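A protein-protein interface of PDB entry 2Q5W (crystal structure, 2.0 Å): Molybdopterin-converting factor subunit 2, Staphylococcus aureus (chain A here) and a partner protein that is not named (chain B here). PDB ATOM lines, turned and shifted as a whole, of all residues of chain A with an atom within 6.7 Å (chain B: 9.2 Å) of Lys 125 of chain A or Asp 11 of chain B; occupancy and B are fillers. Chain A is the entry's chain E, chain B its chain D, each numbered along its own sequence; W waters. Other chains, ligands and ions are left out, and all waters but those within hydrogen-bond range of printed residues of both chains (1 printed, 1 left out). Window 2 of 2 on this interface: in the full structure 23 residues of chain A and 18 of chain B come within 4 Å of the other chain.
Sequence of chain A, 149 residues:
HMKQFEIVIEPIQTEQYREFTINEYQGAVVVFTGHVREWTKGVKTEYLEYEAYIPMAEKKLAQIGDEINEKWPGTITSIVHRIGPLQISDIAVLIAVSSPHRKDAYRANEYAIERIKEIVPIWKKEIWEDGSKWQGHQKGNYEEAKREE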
ATOM      1  N   TYR A  47       6.411  33.302   1.185  1.00  0.00           N
ATOM      2  CA  TYR A  47       6.148  32.701  -0.101  1.00  0.00           C
ATOM      3  C   TYR A  47       4.627  32.785  -0.353  1.00  0.00           C
ATOM      4  O   TYR A  47       3.891  33.228   0.530  1.00  0.00           O
ATOM      5  CB  TYR A  47       6.655  31.241  -0.164  1.00  0.00           C
ATOM      6  CG  TYR A  47       5.978  30.298   0.801  1.00  0.00           C
ATOM      7  CD1 TYR A  47       4.920  29.492   0.396  1.00  0.00           C
ATOM      8  CD2 TYR A  47       6.395  30.217   2.134  1.00  0.00           C
ATOM      9  CE1 TYR A  47       4.290  28.594   1.322  1.00  0.00           C
ATOM     10  CE2 TYR A  47       5.779  29.367   3.032  1.00  0.00           C
ATOM     11  CZ  TYR A  47       4.714  28.566   2.622  1.00  0.00           C
ATOM     12  OH  TYR A  47       4.135  27.716   3.542  1.00  0.00           O
ATOM     13  N   LEU A  48       4.170  32.368  -1.541  1.00  0.00           N
ATOM     14  CA  LEU A  48       2.745  32.282  -1.852  1.00  0.00           C
ATOM     15  C   LEU A  48       2.374  30.822  -2.124  1.00  0.00           C
ATOM     16  O   LEU A  48       3.231  30.034  -2.539  1.00  0.00           O
ATOM     17  CB  LEU A  48       2.372  33.089  -3.092  1.00  0.00           C
ATOM     18  CG  LEU A  48       2.629  34.594  -3.102  1.00  0.00           C
ATOM     19  CD1 LEU A  48       2.041  35.215  -4.372  1.00  0.00           C
ATOM     20  CD2 LEU A  48       2.066  35.240  -1.926  1.00  0.00           C
ATOM     21  N   GLU A  49       1.115  30.454  -1.857  1.00  0.00           N
ATOM     22  CA  GLU A  49       0.562  29.169  -2.279  1.00  0.00           C
ATOM     23  C   GLU A  49      -0.543  29.494  -3.269  1.00  0.00           C
ATOM     24  O   GLU A  49      -1.454  30.243  -2.931  1.00  0.00           O
ATOM     25  CB  GLU A  49      -0.058  28.401  -1.135  1.00  0.00           C
ATOM     26  CG  GLU A  49       0.887  27.931  -0.124  1.00  0.00           C
ATOM     27  CD  GLU A  49       1.182  26.459  -0.223  1.00  0.00           C
ATOM     28  OE1 GLU A  49       1.116  25.859  -1.340  1.00  0.00           O
ATOM     29  OE2 GLU A  49       1.476  25.913   0.855  1.00  0.00           O
ATOM     30  N   TYR A  50      -0.443  28.953  -4.476  1.00  0.00           N
ATOM     31  CA  TYR A  50      -1.509  29.034  -5.442  1.00  0.00           C
ATOM     32  C   TYR A  50      -2.260  27.714  -5.557  1.00  0.00           C
ATOM     33  O   TYR A  50      -1.671  26.626  -5.447  1.00  0.00           O
ATOM     34  CB  TYR A  50      -0.986  29.397  -6.820  1.00  0.00           C
ATOM     35  CG  TYR A  50      -0.658  30.844  -7.029  1.00  0.00           C
ATOM     36  CD1 TYR A  50       0.608  31.339  -6.723  1.00  0.00           C
ATOM     37  CD2 TYR A  50      -1.597  31.714  -7.521  1.00  0.00           C
ATOM     38  CE1 TYR A  50       0.915  32.650  -6.909  1.00  0.00           C
ATOM     39  CE2 TYR A  50      -1.278  33.053  -7.722  1.00  0.00           C
ATOM     40  CZ  TYR A  50      -0.007  33.489  -7.430  1.00  0.00           C
ATOM     41  OH  TYR A  50       0.271  34.820  -7.622  1.00  0.00           O
ATOM     42  N   GLU A  51      -3.555  27.842  -5.797  1.00  0.00           N
ATOM     43  CA  GLU A  51      -4.454  26.743  -6.073  1.00  0.00           C
ATOM     44  C   GLU A  51      -5.211  27.076  -7.358  1.00  0.00           C
ATOM     45  O   GLU A  51      -5.408  28.248  -7.700  1.00  0.00           O
ATOM     46  CB  GLU A  51      -5.517  26.618  -4.978  1.00  0.00           C
ATOM     47  CG  GLU A  51      -5.133  25.799  -3.824  1.00  0.00           C
ATOM     48  CD  GLU A  51      -6.282  25.526  -2.847  1.00  0.00           C
ATOM     49  OE1 GLU A  51      -7.496  25.690  -3.178  1.00  0.00           O
ATOM     50  OE2 GLU A  51      -5.913  25.153  -1.727  1.00  0.00           O
ATOM     51  N   TRP A 123      -6.440  30.836  -7.281  1.00  0.00           N
ATOM     52  CA  TRP A 123      -6.421  31.616  -6.046  1.00  0.00           C
ATOM     53  C   TRP A 123      -5.016  31.683  -5.458  1.00  0.00           C
ATOM     54  O   TRP A 123      -4.269  30.717  -5.534  1.00  0.00           O
ATOM     55  CB  TRP A 123      -7.413  31.057  -5.016  1.00  0.00           C
ATOM     56  CG  TRP A 123      -8.764  30.907  -5.518  1.00  0.00           C
ATOM     57  CD1 TRP A 123      -9.761  31.823  -5.500  1.00  0.00           C
ATOM     58  CD2 TRP A 123      -9.276  29.757  -6.183  1.00  0.00           C
ATOM     59  NE1 TRP A 123     -10.893  31.292  -6.090  1.00  0.00           N
ATOM     60  CE2 TRP A 123     -10.600  30.036  -6.540  1.00  0.00           C
ATOM     61  CE3 TRP A 123      -8.737  28.521  -6.505  1.00  0.00           C
ATOM     62  CZ2 TRP A 123     -11.406  29.114  -7.214  1.00  0.00           C
ATOM     63  CZ3 TRP A 123      -9.533  27.609  -7.212  1.00  0.00           C
ATOM     64  CH2 TRP A 123     -10.845  27.919  -7.551  1.00  0.00           C
ATOM     65  N   LYS A 124      -4.651  32.815  -4.856  1.00  0.00           N
ATOM     66  CA  LYS A 124      -3.406  32.883  -4.103  1.00  0.00           C
ATOM     67  C   LYS A 124      -3.610  33.103  -2.638  1.00  0.00           C
ATOM     68  O   LYS A 124      -4.461  33.909  -2.218  1.00  0.00           O
ATOM     69  CB  LYS A 124      -2.386  33.890  -4.666  1.00  0.00           C
ATOM     70  CG  LYS A 124      -2.741  35.310  -4.768  1.00  0.00           C
ATOM     71  CD  LYS A 124      -1.466  36.242  -4.674  1.00  0.00           C
ATOM     72  CE  LYS A 124      -1.751  37.709  -5.036  1.00  0.00           C
ATOM     73  NZ  LYS A 124      -0.926  38.699  -4.234  1.00  0.00           N
ATOM     74  N   LYS A 125      -2.800  32.398  -1.869  1.00  0.00           N
ATOM     75  CA  LYS A 125      -2.652  32.588  -0.435  1.00  0.00           C
ATOM     76  C   LYS A 125      -1.259  33.181  -0.168  1.00  0.00           C
ATOM     77  O   LYS A 125      -0.257  32.635  -0.639  1.00  0.00           O
ATOM     78  CB  LYS A 125      -2.776  31.242   0.288  1.00  0.00           C
ATOM     79  CG  LYS A 125      -2.949  31.306   1.822  1.00  0.00           C
ATOM     80  CD  LYS A 125      -2.986  29.899   2.425  1.00  0.00           C
ATOM     81  CE  LYS A 125      -3.658  29.866   3.786  1.00  0.00           C
ATOM     82  NZ  LYS A 125      -3.904  28.436   4.254  1.00  0.00           N
ATOM     83  N   GLU A 126      -1.202  34.304   0.540  1.00  0.00           N
ATOM     84  CA  GLU A 126       0.048  34.858   1.055  1.00  0.00           C
ATOM     85  C   GLU A 126       0.372  34.267   2.393  1.00  0.00           C
ATOM     86  O   GLU A 126      -0.508  34.195   3.276  1.00  0.00           O
ATOM     87  CB  GLU A 126      -0.030  36.378   1.268  1.00  0.00           C
ATOM     88  CG  GLU A 126      -0.275  37.098   0.013  1.00  0.00           C
ATOM     89  CD  GLU A 126       0.024  38.587   0.070  1.00  0.00           C
ATOM     90  OE1 GLU A 126       0.440  39.110   1.119  1.00  0.00           O
ATOM     91  OE2 GLU A 126      -0.187  39.209  -0.993  1.00  0.00           O
ATOM     92  N   ILE A 127       1.638  33.878   2.556  1.00  0.00           N
ATOM     93  CA  ILE A 127       2.129  33.340   3.817  1.00  0.00           C
ATOM     94  C   ILE A 127       3.221  34.254   4.377  1.00  0.00           C
ATOM     95  O   ILE A 127       4.159  34.631   3.674  1.00  0.00           O
ATOM     96  CB  ILE A 127       2.668  31.901   3.657  1.00  0.00           C
ATOM     97  CG1 ILE A 127       1.523  30.911   3.358  1.00  0.00           C
ATOM     98  CG2 ILE A 127       3.320  31.429   4.969  1.00  0.00           C
ATOM     99  CD1 ILE A 127       1.247  30.690   2.062  1.00  0.00           C
ATOM    100  N   SER A 132      -1.245  33.839   7.390  1.00  0.00           N
ATOM    101  CA  SER A 132      -1.490  33.594   5.983  1.00  0.00           C
ATOM    102  C   SER A 132      -2.888  34.083   5.685  1.00  0.00           C
ATOM    103  O   SER A 132      -3.732  34.109   6.592  1.00  0.00           O
ATOM    104  CB  SER A 132      -1.388  32.110   5.711  1.00  0.00           C
ATOM    105  OG  SER A 132      -2.402  31.419   6.413  1.00  0.00           O
ATOM    106  N   LYS A 133      -3.141  34.485   4.449  1.00  0.00           N
ATOM    107  CA  LYS A 133      -4.446  34.958   4.048  1.00  0.00           C
ATOM    108  C   LYS A 133      -4.682  34.708   2.553  1.00  0.00           C
ATOM    109  O   LYS A 133      -3.856  35.077   1.715  1.00  0.00           O
ATOM    110  CB  LYS A 133      -4.589  36.448   4.334  1.00  0.00           C
ATOM    111  CG  LYS A 133      -5.957  37.050   3.888  1.00  0.00           C
ATOM    112  CD  LYS A 133      -6.434  38.208   4.780  1.00  0.00           C
ATOM    113  CE  LYS A 133      -7.960  38.446   4.666  1.00  0.00           C
ATOM    114  NZ  LYS A 133      -8.506  39.291   5.792  1.00  0.00           N
ATOM    115  N   TRP A 134      -5.806  34.073   2.231  1.00  0.00           N
ATOM    116  CA  TRP A 134      -6.252  33.969   0.852  1.00  0.00           C
ATOM    117  C   TRP A 134      -6.592  35.361   0.330  1.00  0.00           C
ATOM    118  O   TRP A 134      -7.306  36.130   0.987  1.00  0.00           O
ATOM    119  CB  TRP A 134      -7.480  33.043   0.733  1.00  0.00           C
ATOM    120  CG  TRP A 134      -7.122  31.632   0.920  1.00  0.00           C
ATOM    121  CD1 TRP A 134      -7.321  30.887   2.028  1.00  0.00           C
ATOM    122  CD2 TRP A 134      -6.468  30.788  -0.020  1.00  0.00           C
ATOM    123  NE1 TRP A 134      -6.834  29.626   1.838  1.00  0.00           N
ATOM    124  CE2 TRP A 134      -6.309  29.534   0.585  1.00  0.00           C
ATOM    125  CE3 TRP A 134      -6.012  30.968  -1.325  1.00  0.00           C
ATOM    126  CZ2 TRP A 134      -5.694  28.472  -0.052  1.00  0.00           C
ATOM    127  CZ3 TRP A 134      -5.403  29.916  -1.960  1.00  0.00           C
ATOM    128  CH2 TRP A 134      -5.252  28.688  -1.331  1.00  0.00           C
ATOM    129  N   GLN A 135      -6.077  35.686  -0.850  1.00  0.00           N
ATOM    130  CA  GLN A 135      -6.350  36.976  -1.472  1.00  0.00           C
ATOM    131  C   GLN A 135      -7.625  36.881  -2.318  1.00  0.00           C
ATOM    132  O   GLN A 135      -7.983  35.809  -2.839  1.00  0.00           O
ATOM    133  CB  GLN A 135      -5.150  37.425  -2.305  1.00  0.00           C
ATOM    134  CG  GLN A 135      -3.766  37.308  -1.548  1.00  0.00           C
ATOM    135  CD  GLN A 135      -3.673  38.238  -0.321  1.00  0.00           C
ATOM    136  OE1 GLN A 135      -3.440  37.793   0.813  1.00  0.00           O
ATOM    137  NE2 GLN A 135      -3.889  39.539  -0.555  1.00  0.00           N
ATOM    138  N   TYR B   5     -14.152  21.833  -3.296  1.00  0.00           N
ATOM    139  CA  TYR B   5     -13.937  23.041  -2.501  1.00  0.00           C
ATOM    140  C   TYR B   5     -12.518  23.538  -2.740  1.00  0.00           C
ATOM    141  O   TYR B   5     -11.576  22.752  -2.869  1.00  0.00           O
ATOM    142  CB  TYR B   5     -14.093  22.736  -1.022  1.00  0.00           C
ATOM    143  CG  TYR B   5     -15.408  22.127  -0.651  1.00  0.00           C
ATOM    144  CD1 TYR B   5     -15.503  20.809  -0.209  1.00  0.00           C
ATOM    145  CD2 TYR B   5     -16.567  22.858  -0.756  1.00  0.00           C
ATOM    146  CE1 TYR B   5     -16.731  20.265   0.151  1.00  0.00           C
ATOM    147  CE2 TYR B   5     -17.790  22.325  -0.405  1.00  0.00           C
ATOM    148  CZ  TYR B   5     -17.867  21.034   0.037  1.00  0.00           C
ATOM    149  OH  TYR B   5     -19.106  20.556   0.371  1.00  0.00           O
ATOM    150  N   PHE B   6     -12.381  24.864  -2.752  1.00  0.00           N
ATOM    151  CA  PHE B   6     -11.129  25.550  -3.079  1.00  0.00           C
ATOM    152  C   PHE B   6     -10.886  26.687  -2.110  1.00  0.00           C
ATOM    153  O   PHE B   6     -11.815  27.271  -1.567  1.00  0.00           O
ATOM    154  CB  PHE B   6     -11.157  26.078  -4.549  1.00  0.00           C
ATOM    155  CG  PHE B   6     -11.241  24.974  -5.555  1.00  0.00           C
ATOM    156  CD1 PHE B   6     -12.471  24.501  -5.982  1.00  0.00           C
ATOM    157  CD2 PHE B   6     -10.101  24.307  -5.949  1.00  0.00           C
ATOM    158  CE1 PHE B   6     -12.561  23.393  -6.848  1.00  0.00           C
ATOM    159  CE2 PHE B   6     -10.187  23.234  -6.843  1.00  0.00           C
ATOM    160  CZ  PHE B   6     -11.429  22.770  -7.261  1.00  0.00           C
ATOM    161  N   ALA B   7      -9.606  26.960  -1.890  1.00  0.00           N
ATOM    162  CA  ALA B   7      -9.147  28.187  -1.249  1.00  0.00           C
ATOM    163  C   ALA B   7      -9.687  28.299   0.156  1.00  0.00           C
ATOM    164  O   ALA B   7      -9.645  27.314   0.890  1.00  0.00           O
ATOM    165  CB  ALA B   7      -9.464  29.403  -2.124  1.00  0.00           C
ATOM    166  N   GLU B   8     -10.212  29.453   0.556  1.00  0.00           N
ATOM    167  CA  GLU B   8     -10.582  29.604   1.956  1.00  0.00           C
ATOM    168  C   GLU B   8     -11.684  28.615   2.418  1.00  0.00           C
ATOM    169  O   GLU B   8     -11.640  28.113   3.556  1.00  0.00           O
ATOM    170  CB  GLU B   8     -10.957  31.039   2.272  1.00  0.00           C
ATOM    171  CG  GLU B   8     -11.189  31.254   3.743  1.00  0.00           C
ATOM    172  CD  GLU B   8     -11.665  32.634   4.048  1.00  0.00           C
ATOM    173  OE1 GLU B   8     -12.018  33.367   3.094  1.00  0.00           O
ATOM    174  OE2 GLU B   8     -11.711  32.978   5.242  1.00  0.00           O
ATOM    175  N   ILE B   9     -12.632  28.311   1.536  1.00  0.00           N
ATOM    176  CA  ILE B   9     -13.712  27.384   1.866  1.00  0.00           C
ATOM    177  C   ILE B   9     -13.159  25.979   2.151  1.00  0.00           C
ATOM    178  O   ILE B   9     -13.515  25.353   3.166  1.00  0.00           O
ATOM    179  CB  ILE B   9     -14.804  27.357   0.765  1.00  0.00           C
ATOM    180  CG1 ILE B   9     -15.575  28.692   0.822  1.00  0.00           C
ATOM    181  CG2 ILE B   9     -15.725  26.164   0.979  1.00  0.00           C
ATOM    182  CD1 ILE B   9     -16.442  28.973  -0.363  1.00  0.00           C
ATOM    183  N   LYS B  10     -12.253  25.537   1.290  1.00  0.00           N
ATOM    184  CA  LYS B  10     -11.500  24.318   1.505  1.00  0.00           C
ATOM    185  C   LYS B  10     -10.813  24.315   2.880  1.00  0.00           C
ATOM    186  O   LYS B  10     -10.903  23.323   3.633  1.00  0.00           O
ATOM    187  CB  LYS B  10     -10.515  24.103   0.331  1.00  0.00           C
ATOM    188  CG  LYS B  10      -9.586  22.925   0.443  1.00  0.00           C
ATOM    189  CD  LYS B  10      -8.749  22.835  -0.829  1.00  0.00           C
ATOM    190  CE  LYS B  10      -7.341  22.394  -0.532  1.00  0.00           C
ATOM    191  NZ  LYS B  10      -6.584  22.070  -1.776  1.00  0.00           N
ATOM    192  N   ASP B  11     -10.175  25.427   3.228  1.00  0.00           N
ATOM    193  CA  ASP B  11      -9.481  25.514   4.493  1.00  0.00           C
ATOM    194  C   ASP B  11     -10.462  25.397   5.656  1.00  0.00           C
ATOM    195  O   ASP B  11     -10.214  24.692   6.626  1.00  0.00           O
ATOM    196  CB  ASP B  11      -8.742  26.843   4.615  1.00  0.00           C
ATOM    197  CG  ASP B  11      -7.399  26.824   3.944  1.00  0.00           C
ATOM    198  OD1 ASP B  11      -7.039  25.793   3.332  1.00  0.00           O
ATOM    199  OD2 ASP B  11      -6.702  27.845   4.059  1.00  0.00           O
ATOM    200  N   ILE B  12     -11.583  26.108   5.547  1.00  0.00           N
ATOM    201  CA  ILE B  12     -12.580  26.118   6.598  1.00  0.00           C
ATOM    202  C   ILE B  12     -13.215  24.735   6.761  1.00  0.00           C
ATOM    203  O   ILE B  12     -13.282  24.213   7.862  1.00  0.00           O
ATOM    204  CB  ILE B  12     -13.657  27.196   6.346  1.00  0.00           C
ATOM    205  CG1 ILE B  12     -13.032  28.582   6.509  1.00  0.00           C
ATOM    206  CG2 ILE B  12     -14.787  27.048   7.375  1.00  0.00           C
ATOM    207  CD1 ILE B  12     -13.875  29.703   5.918  1.00  0.00           C
ATOM    208  N   LEU B  13     -13.643  24.124   5.660  1.00  0.00           N
ATOM    209  CA  LEU B  13     -14.262  22.801   5.744  1.00  0.00           C
ATOM    210  C   LEU B  13     -13.266  21.666   6.029  1.00  0.00           C
ATOM    211  O   LEU B  13     -13.663  20.580   6.418  1.00  0.00           O
ATOM    212  CB  LEU B  13     -15.078  22.527   4.492  1.00  0.00           C
ATOM    213  CG  LEU B  13     -16.151  23.570   4.135  1.00  0.00           C
ATOM    214  CD1 LEU B  13     -16.934  23.108   2.906  1.00  0.00           C
ATOM    215  CD2 LEU B  13     -17.094  23.800   5.271  1.00  0.00           C
ATOM    216  N   GLN B  14     -11.975  21.943   5.894  1.00  0.00           N
ATOM    217  CA  GLN B  14     -10.904  20.945   6.058  1.00  0.00           C
ATOM    218  C   GLN B  14     -11.124  19.753   5.114  1.00  0.00           C
ATOM    219  O   GLN B  14     -10.883  18.623   5.448  1.00  0.00           O
ATOM    220  CB  GLN B  14     -10.783  20.495   7.514  1.00  0.00           C
ATOM    221  CG  GLN B  14     -10.354  21.596   8.477  1.00  0.00           C
ATOM    222  CD  GLN B  14     -10.378  21.131   9.936  1.00  0.00           C
ATOM    223  OE1 GLN B  14     -11.320  21.411  10.693  1.00  0.00           O
ATOM    224  NE2 GLN B  14      -9.358  20.394  10.326  1.00  0.00           N
ATOM    225  N   LYS B  15     -11.614  20.023   3.911  1.00  0.00           N
ATOM    226  CA  LYS B  15     -11.796  18.954   2.952  1.00  0.00           C
ATOM    227  C   LYS B  15     -11.842  19.574   1.560  1.00  0.00           C
ATOM    228  O   LYS B  15     -12.298  20.713   1.371  1.00  0.00           O
ATOM    229  CB  LYS B  15     -13.042  18.088   3.294  1.00  0.00           C
ATOM    230  CG  LYS B  15     -14.364  18.758   2.927  1.00  0.00           C
ATOM    231  CD  LYS B  15     -15.563  17.959   3.386  1.00  0.00           C
ATOM    232  CE  LYS B  15     -15.919  18.214   4.825  1.00  0.00           C
ATOM    233  NZ  LYS B  15     -17.102  17.428   5.239  1.00  0.00           N
ATOM    234  N   ALA B  16     -11.333  18.822   0.593  1.00  0.00           N
ATOM    235  CA  ALA B  16     -11.273  19.304  -0.781  1.00  0.00           C
ATOM    236  C   ALA B  16     -12.420  18.770  -1.639  1.00  0.00           C
ATOM    237  O   ALA B  16     -12.753  19.331  -2.668  1.00  0.00           O
ATOM    238  CB  ALA B  16      -9.969  18.973  -1.388  1.00  0.00           C
ATOM    239  N   GLN B  41     -20.638  27.652   9.125  1.00  0.00           N
ATOM    240  CA  GLN B  41     -19.365  28.361   9.169  1.00  0.00           C
ATOM    241  C   GLN B  41     -18.917  28.923   7.823  1.00  0.00           C
ATOM    242  O   GLN B  41     -17.982  29.717   7.783  1.00  0.00           O
ATOM    243  CB  GLN B  41     -18.264  27.475   9.764  1.00  0.00           C
ATOM    244  CG  GLN B  41     -17.913  26.226   8.925  1.00  0.00           C
ATOM    245  CD  GLN B  41     -18.711  24.987   9.343  1.00  0.00           C
ATOM    246  OE1 GLN B  41     -19.898  25.060   9.674  1.00  0.00           O
ATOM    247  NE2 GLN B  41     -18.051  23.860   9.344  1.00  0.00           N
ATOM    248  N   ILE B  42     -19.527  28.512   6.723  1.00  0.00           N
ATOM    249  CA  ILE B  42     -19.275  29.217   5.456  1.00  0.00           C
ATOM    250  C   ILE B  42     -20.435  30.077   4.982  1.00  0.00           C
ATOM    251  O   ILE B  42     -20.377  30.611   3.896  1.00  0.00           O
ATOM    252  CB  ILE B  42     -18.834  28.278   4.290  1.00  0.00           C
ATOM    253  CG1 ILE B  42     -19.962  27.318   3.907  1.00  0.00           C
ATOM    254  CG2 ILE B  42     -17.522  27.551   4.644  1.00  0.00           C
ATOM    255  CD1 ILE B  42     -19.684  26.602   2.620  1.00  0.00           C
ATOM    256  N   LYS B  45     -19.687  33.356   3.258  1.00  0.00           N
ATOM    257  CA  LYS B  45     -18.573  33.381   2.307  1.00  0.00           C
ATOM    258  C   LYS B  45     -19.116  33.624   0.901  1.00  0.00           C
ATOM    259  O   LYS B  45     -20.200  33.160   0.554  1.00  0.00           O
ATOM    260  CB  LYS B  45     -17.739  32.092   2.370  1.00  0.00           C
ATOM    261  CG  LYS B  45     -17.039  31.892   3.710  1.00  0.00           C
ATOM    262  CD  LYS B  45     -15.976  32.953   3.981  1.00  0.00           C
ATOM    263  CE  LYS B  45     -15.534  32.946   5.400  1.00  0.00           C
ATOM    264  NZ  LYS B  45     -14.570  34.069   5.685  1.00  0.00           N
ATOM    265  N   PRO B  72     -14.541  30.670  -4.975  1.00  0.00           N
ATOM    266  CA  PRO B  72     -14.443  31.969  -4.316  1.00  0.00           C
ATOM    267  C   PRO B  72     -13.868  33.029  -5.236  1.00  0.00           C
ATOM    268  O   PRO B  72     -13.463  32.709  -6.370  1.00  0.00           O
ATOM    269  CB  PRO B  72     -13.520  31.703  -3.119  1.00  0.00           C
ATOM    270  CG  PRO B  72     -13.496  30.230  -2.957  1.00  0.00           C
ATOM    271  CD  PRO B  72     -13.700  29.668  -4.342  1.00  0.00           C
ATOM    272  N   SER B  75      -8.114  35.170  -7.684  1.00  0.00           N
ATOM    273  CA  SER B  75      -6.947  36.015  -7.369  1.00  0.00           C
ATOM    274  C   SER B  75      -5.684  35.475  -8.087  1.00  0.00           C
ATOM    275  O   SER B  75      -4.551  35.581  -7.582  1.00  0.00           O
ATOM    276  CB  SER B  75      -6.754  36.081  -5.845  1.00  0.00           C
ATOM    277  OG  SER B  75      -6.558  34.791  -5.271  1.00  0.00           O
ATOM    278  N   GLY B  76      -5.883  34.923  -9.292  1.00  0.00           N
ATOM    279  CA  GLY B  76      -4.771  34.552 -10.130  1.00  0.00           C
ATOM    280  C   GLY B  76      -4.146  35.722 -10.855  1.00  0.00           C
ATOM    281  O   GLY B  76      -4.675  36.844 -10.832  1.00  0.00           O
HETATM  282  O   HOH W   1      -1.907  36.467  -8.226  1.00  0.00           O
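The side-chain amino group (NZ) of Lys 125 of chain A lies within salt-bridge range of the side-chain carboxylate (OD2) of Asp 11 of chain B (2.9 Å). The side-chain carboxylate of Glu 51 of chain A lies within salt-bridge range of the side-chain amino group of Lys 10 of chain B (3.2 Å). The side-chain carboxylate of Glu 51 of chain A lies within hydrogen-bond range of the backbone NH of Ala 7 of chain B (2.8 Å). The backbone carbonyl oxygen (O) of Gln 135 of chain A is in hydrogen-bond range of the side-chain hydroxyl (OG) of Ser 75 of chain B (3.0 Å). N of Lys 124 of chain A lies within hydrogen-bond range of OG of Ser 75 of chain B. NE1 of Trp 123 of chain A lies within hydrogen-bond range of O of Pro 72 of chain B, at 2.9 Å. The indole nitrogen (NE1) of Trp 134 of chain A is in hydrogen-bond range of the side-chain carboxylate (OD2) of Asp 11 of chain B, 2.8 Å away.
The backbone carbonyl oxygen (O) of Lys 124 of chain A is in hydrogen-bond range of the backbone NH (N) of Gln 135 of chain A (2.8 Å). The backbone NH (N) of Trp 123 of chain A lies within hydrogen-bond range of the backbone carbonyl oxygen (O) of Glu 51 of chain A. The backbone carbonyl oxygen of Lys 133 of chain A sits close to the side-chain amide oxygen of Gln 135 of chain A (2.9 Å). The side-chain amino group (NZ) of Lys 45 of chain B lies within salt-bridge range of the side-chain carboxylate (OE2) of Glu 8 of chain B, at 3.1 Å. The side-chain carboxylate (OE2) of Glu 126 of chain A is in salt-bridge range of the side-chain amino group (NZ) of Lys 124 of chain A, 3.4 Å away. The backbone carbonyl oxygen of Glu 49 of chain A sits at hydrogen-bond distance from the backbone NH of Lys 125 of chain A.
Among the printed residues, pairs that only touch across the chains: Glu 51 of chain A with Phe 6 of chain B (3.6 Å), Trp 123 of chain A with Phe 6 of chain B (3.5 Å), Trp 123 of chain A with Ala 7 of chain B (3.8 Å), Trp 123 of chain A with Ser 75 of chain B (3.3 Å), Trp 134 of chain A with Ala 7 of chain B (3.6 Å) and Trp 134 of chain A with Glu 8 of chain B (3.5 Å).
No residue of chain B comes within 4 Å of Leu 48 of chain A. Printed residues of chain B within 4 Å of Glu 51 of chain A: Phe 6 (3.6 Å), Ala 7 (2.8 Å) and Lys 10 (3.2 Å). Of the printed residues of chain A, Ala 7 of chain B touches Glu 51 (2.8 Å), Trp 123 (3.8 Å) and Trp 134 (3.6 Å). Printed residues of chain A within 4 Å of Glu 8 of chain B: Trp 134. The nearest residue of chain A that does not touch Asp 11 of chain B is Glu 51 of chain A (5.2 Å).
Hydrophobic or aromatic side chains of chain A that line the printed part of chain B: Trp 123 and Trp 134. Among the printed residues, 13 pairs touch across the chains.
Water W1 bridges OH of Tyr 50 of chain A (2.8 Å) and O of Ser 75 of chain B (2.9 Å).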
